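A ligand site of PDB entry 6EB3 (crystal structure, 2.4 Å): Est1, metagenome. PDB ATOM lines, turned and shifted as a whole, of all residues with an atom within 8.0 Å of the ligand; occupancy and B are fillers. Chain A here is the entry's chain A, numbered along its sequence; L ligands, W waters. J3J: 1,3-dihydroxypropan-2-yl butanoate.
The side-chain amide oxygen of Gln 48 sits at hydrogen-bond distance from an oxygen (O2) of the ligand (2.9 Å). The backbone carbonyl oxygen (O) of Gly 17 is in hydrogen-bond range of an oxygen (O2) of the ligand. O1 of the ligand lies within hydrogen-bond range of O of Ile 15 (3.2 Å).
CA of Glu 16 touches C3 of the ligand, 3.8 Å away. Gln 18 touches the ligand. Along chain A the residues within 4 Å of the ligand span positions 15 to 48.
Water W2 lies within hydrogen-bond range of an oxygen (O1) of the ligand (2.7 Å), the side-chain carboxylate of Glu 16 (2.9 Å) and the backbone carbonyl oxygen of Ile 15 (3.4 Å).
O of Gln 18 sits close to N of His 47 (3.5 Å). O of Glu 16 lies within hydrogen-bond range of N of Val 49, at 2.8 Å.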
ATOM      1  N   LEU A   2       6.947  24.624  -3.664  1.00  0.00           N
ATOM      2  CA  LEU A   2       7.865  24.483  -4.809  1.00  0.00           C
ATOM      3  C   LEU A   2       7.732  25.584  -5.835  1.00  0.00           C
ATOM      4  O   LEU A   2       6.618  25.989  -6.163  1.00  0.00           O
ATOM      5  CB  LEU A   2       7.639  23.150  -5.526  1.00  0.00           C
ATOM      6  CG  LEU A   2       7.881  21.908  -4.694  1.00  0.00           C
ATOM      7  CD1 LEU A   2       7.459  20.671  -5.468  1.00  0.00           C
ATOM      8  CD2 LEU A   2       9.344  21.839  -4.265  1.00  0.00           C
ATOM      9  N   TYR A  13       4.342  25.735  -8.564  1.00  0.00           N
ATOM     10  CA  TYR A  13       3.738  24.559  -9.190  1.00  0.00           C
ATOM     11  C   TYR A  13       3.600  23.441  -8.166  1.00  0.00           C
ATOM     12  O   TYR A  13       4.239  23.459  -7.109  1.00  0.00           O
ATOM     13  CB  TYR A  13       4.556  24.051 -10.402  1.00  0.00           C
ATOM     14  CG  TYR A  13       5.864  23.394 -10.004  1.00  0.00           C
ATOM     15  CD1 TYR A  13       6.996  24.168  -9.734  1.00  0.00           C
ATOM     16  CD2 TYR A  13       5.958  22.030  -9.858  1.00  0.00           C
ATOM     17  CE1 TYR A  13       8.184  23.579  -9.358  1.00  0.00           C
ATOM     18  CE2 TYR A  13       7.142  21.436  -9.459  1.00  0.00           C
ATOM     19  CZ  TYR A  13       8.267  22.229  -9.220  1.00  0.00           C
ATOM     20  OH  TYR A  13       9.463  21.683  -8.833  1.00  0.00           O
ATOM     21  N   GLU A  14       2.765  22.460  -8.508  1.00  0.00           N
ATOM     22  CA  GLU A  14       2.708  21.196  -7.798  1.00  0.00           C
ATOM     23  C   GLU A  14       2.750  20.099  -8.829  1.00  0.00           C
ATOM     24  O   GLU A  14       2.166  20.241  -9.902  1.00  0.00           O
ATOM     25  CB  GLU A  14       1.411  21.088  -6.973  1.00  0.00           C
ATOM     26  CG  GLU A  14       1.328  22.137  -5.882  1.00  0.00           C
ATOM     27  CD  GLU A  14      -0.062  22.259  -5.254  1.00  0.00           C
ATOM     28  OE1 GLU A  14      -0.857  21.282  -5.259  1.00  0.00           O
ATOM     29  OE2 GLU A  14      -0.378  23.351  -4.726  1.00  0.00           O
ATOM     30  N   ILE A  15       3.389  18.997  -8.486  1.00  0.00           N
ATOM     31  CA  ILE A  15       3.501  17.851  -9.377  1.00  0.00           C
ATOM     32  C   ILE A  15       3.195  16.592  -8.563  1.00  0.00           C
ATOM     33  O   ILE A  15       3.666  16.462  -7.439  1.00  0.00           O
ATOM     34  CB  ILE A  15       4.874  17.840 -10.068  1.00  0.00           C
ATOM     35  CG1 ILE A  15       4.995  16.659 -11.037  1.00  0.00           C
ATOM     36  CG2 ILE A  15       6.021  17.789  -9.083  1.00  0.00           C
ATOM     37  CD1 ILE A  15       6.168  16.794 -11.979  1.00  0.00           C
ATOM     38  N   GLU A  16       2.371  15.705  -9.124  1.00  0.00           N
ATOM     39  CA  GLU A  16       1.910  14.518  -8.426  1.00  0.00           C
ATOM     40  C   GLU A  16       1.601  13.410  -9.420  1.00  0.00           C
ATOM     41  O   GLU A  16       1.082  13.648 -10.508  1.00  0.00           O
ATOM     42  CB  GLU A  16       0.618  14.835  -7.639  1.00  0.00           C
ATOM     43  CG  GLU A  16       0.186  13.965  -6.447  1.00  0.00           C
ATOM     44  CD  GLU A  16       1.294  13.609  -5.441  1.00  0.00           C
ATOM     45  OE1 GLU A  16       1.828  12.511  -5.707  1.00  0.00           O
ATOM     46  OE2 GLU A  16       1.675  14.382  -4.504  1.00  0.00           O
ATOM     47  N   GLY A  17       1.920  12.201  -9.001  1.00  0.00           N
ATOM     48  CA  GLY A  17       1.576  10.998  -9.713  1.00  0.00           C
ATOM     49  C   GLY A  17       2.766  10.499 -10.497  1.00  0.00           C
ATOM     50  O   GLY A  17       3.817  11.148 -10.581  1.00  0.00           O
ATOM     51  N   GLN A  18       2.575   9.313 -11.062  1.00  0.00           N
ATOM     52  CA  GLN A  18       3.529   8.672 -11.921  1.00  0.00           C
ATOM     53  C   GLN A  18       2.850   8.380 -13.243  1.00  0.00           C
ATOM     54  O   GLN A  18       1.637   8.209 -13.301  1.00  0.00           O
ATOM     55  CB  GLN A  18       4.027   7.370 -11.280  1.00  0.00           C
ATOM     56  CG  GLN A  18       4.716   7.528  -9.897  1.00  0.00           C
ATOM     57  CD  GLN A  18       5.912   8.527  -9.859  1.00  0.00           C
ATOM     58  OE1 GLN A  18       6.214   9.149  -8.824  1.00  0.00           O
ATOM     59  NE2 GLN A  18       6.629   8.641 -10.978  1.00  0.00           N
ATOM     60  N   GLY A  19       3.655   8.337 -14.288  1.00  0.00           N
ATOM     61  CA  GLY A  19       3.170   8.114 -15.622  1.00  0.00           C
ATOM     62  C   GLY A  19       3.653   9.226 -16.519  1.00  0.00           C
ATOM     63  O   GLY A  19       4.547   9.994 -16.154  1.00  0.00           O
ATOM     64  N   THR A  44      -3.935  11.793 -11.380  1.00  0.00           N
ATOM     65  CA  THR A  44      -2.666  11.335 -10.798  1.00  0.00           C
ATOM     66  C   THR A  44      -2.515   9.809 -10.745  1.00  0.00           C
ATOM     67  O   THR A  44      -1.406   9.304 -10.669  1.00  0.00           O
ATOM     68  CB  THR A  44      -2.403  11.882  -9.357  1.00  0.00           C
ATOM     69  OG1 THR A  44      -3.411  11.362  -8.456  1.00  0.00           O
ATOM     70  CG2 THR A  44      -2.378  13.428  -9.296  1.00  0.00           C
ATOM     71  N   HIS A  47      -1.305   9.459 -14.647  1.00  0.00           N
ATOM     72  CA  HIS A  47      -0.381  10.403 -15.233  1.00  0.00           C
ATOM     73  C   HIS A  47       0.354  11.151 -14.137  1.00  0.00           C
ATOM     74  O   HIS A  47      -0.082  11.202 -12.979  1.00  0.00           O
ATOM     75  CB  HIS A  47      -1.156  11.365 -16.154  1.00  0.00           C
ATOM     76  CG  HIS A  47      -1.663  10.727 -17.404  1.00  0.00           C
ATOM     77  ND1 HIS A  47      -2.821   9.970 -17.442  1.00  0.00           N
ATOM     78  CD2 HIS A  47      -1.152  10.673 -18.665  1.00  0.00           C
ATOM     79  CE1 HIS A  47      -3.022   9.513 -18.666  1.00  0.00           C
ATOM     80  NE2 HIS A  47      -2.018   9.917 -19.425  1.00  0.00           N
ATOM     81  N   GLN A  48       1.506  11.694 -14.498  1.00  0.00           N
ATOM     82  CA  GLN A  48       2.201  12.662 -13.682  1.00  0.00           C
ATOM     83  C   GLN A  48       1.606  14.054 -14.002  1.00  0.00           C
ATOM     84  O   GLN A  48       1.867  14.614 -15.043  1.00  0.00           O
ATOM     85  CB  GLN A  48       3.700  12.606 -13.952  1.00  0.00           C
ATOM     86  CG  GLN A  48       4.479  13.747 -13.309  1.00  0.00           C
ATOM     87  CD  GLN A  48       5.942  13.451 -13.234  1.00  0.00           C
ATOM     88  OE1 GLN A  48       6.363  12.884 -12.256  1.00  0.00           O
ATOM     89  NE2 GLN A  48       6.737  13.886 -14.224  1.00  0.00           N
ATOM     90  N   VAL A  49       0.776  14.572 -13.095  1.00  0.00           N
ATOM     91  CA  VAL A  49       0.000  15.778 -13.315  1.00  0.00           C
ATOM     92  C   VAL A  49       0.763  16.974 -12.786  1.00  0.00           C
ATOM     93  O   VAL A  49       1.206  16.981 -11.636  1.00  0.00           O
ATOM     94  CB  VAL A  49      -1.344  15.707 -12.583  1.00  0.00           C
ATOM     95  CG1 VAL A  49      -2.164  16.960 -12.829  1.00  0.00           C
ATOM     96  CG2 VAL A  49      -2.130  14.477 -13.030  1.00  0.00           C
ATOM     97  N   ILE A  50       0.874  17.994 -13.625  1.00  0.00           N
ATOM     98  CA  ILE A  50       1.491  19.248 -13.250  1.00  0.00           C
ATOM     99  C   ILE A  50       0.448  20.358 -13.277  1.00  0.00           C
ATOM    100  O   ILE A  50      -0.164  20.606 -14.322  1.00  0.00           O
ATOM    101  CB  ILE A  50       2.623  19.607 -14.222  1.00  0.00           C
ATOM    102  CG1 ILE A  50       3.657  18.492 -14.294  1.00  0.00           C
ATOM    103  CG2 ILE A  50       3.302  20.912 -13.779  1.00  0.00           C
ATOM    104  CD1 ILE A  50       4.361  18.433 -15.596  1.00  0.00           C
ATOM    105  N   LEU A  83      11.574  21.391 -14.973  1.00  0.00           N
ATOM    106  CA  LEU A  83      11.248  20.011 -14.553  1.00  0.00           C
ATOM    107  C   LEU A  83      11.914  18.958 -15.434  1.00  0.00           C
ATOM    108  O   LEU A  83      11.739  17.760 -15.203  1.00  0.00           O
ATOM    109  CB  LEU A  83       9.736  19.813 -14.586  1.00  0.00           C
ATOM    110  CG  LEU A  83       8.926  20.682 -13.612  1.00  0.00           C
ATOM    111  CD1 LEU A  83       7.435  20.628 -13.924  1.00  0.00           C
ATOM    112  CD2 LEU A  83       9.210  20.245 -12.175  1.00  0.00           C
ATOM    113  N   ASN A  84      12.676  19.397 -16.441  1.00  0.00           N
ATOM    114  CA  ASN A  84      13.351  18.513 -17.352  1.00  0.00           C
ATOM    115  C   ASN A  84      12.366  17.525 -18.012  1.00  0.00           C
ATOM    116  O   ASN A  84      12.615  16.329 -18.058  1.00  0.00           O
ATOM    117  CB  ASN A  84      14.491  17.773 -16.610  1.00  0.00           C
ATOM    118  CG  ASN A  84      15.497  17.153 -17.570  1.00  0.00           C
ATOM    119  OD1 ASN A  84      15.712  17.655 -18.665  1.00  0.00           O
ATOM    120  ND2 ASN A  84      16.104  16.026 -17.165  1.00  0.00           N
ATOM    121  N   ILE A  85      11.240  18.042 -18.487  1.00  0.00           N
ATOM    122  CA  ILE A  85      10.246  17.269 -19.250  1.00  0.00           C
ATOM    123  C   ILE A  85      10.320  17.709 -20.720  1.00  0.00           C
ATOM    124  O   ILE A  85       9.939  18.832 -21.059  1.00  0.00           O
ATOM    125  CB  ILE A  85       8.822  17.436 -18.669  1.00  0.00           C
ATOM    126  CG1 ILE A  85       8.739  16.856 -17.247  1.00  0.00           C
ATOM    127  CG2 ILE A  85       7.774  16.802 -19.567  1.00  0.00           C
ATOM    128  CD1 ILE A  85       7.610  17.374 -16.423  1.00  0.00           C
HETATM  129  O1  J3J L   1       5.909  14.749  -5.920  1.00  0.00           O
HETATM  130  C1  J3J L   1       6.770  13.618  -6.131  1.00  0.00           C
HETATM  131  C2  J3J L   1       6.851  13.195  -7.602  1.00  0.00           C
HETATM  132  C3  J3J L   1       5.425  13.028  -8.143  1.00  0.00           C
HETATM  133  O2  J3J L   1       5.406  12.834  -9.568  1.00  0.00           O
HETATM  134  O3  J3J L   1       7.618  14.147  -8.360  1.00  0.00           O
HETATM  135  C4  J3J L   1       8.961  13.708  -8.790  1.00  0.00           C
HETATM  136  O4  J3J L   1       9.943  14.146  -8.211  1.00  0.00           O
HETATM  137  C5  J3J L   1       9.140  12.717  -9.936  1.00  0.00           C
HETATM  138  C6  J3J L   1       9.844  13.370 -11.126  1.00  0.00           C
HETATM  139  C7  J3J L   1       9.929  12.428 -12.319  1.00  0.00           C
HETATM  140  O   HOH W   1       9.960  13.601  -5.047  1.00  0.00           O
HETATM  141  O   HOH W   2       4.112  15.839  -4.150  1.00  0.00           O
HETATM  142  O   HOH W   3       6.560  17.039  -5.171  1.00  0.00           O
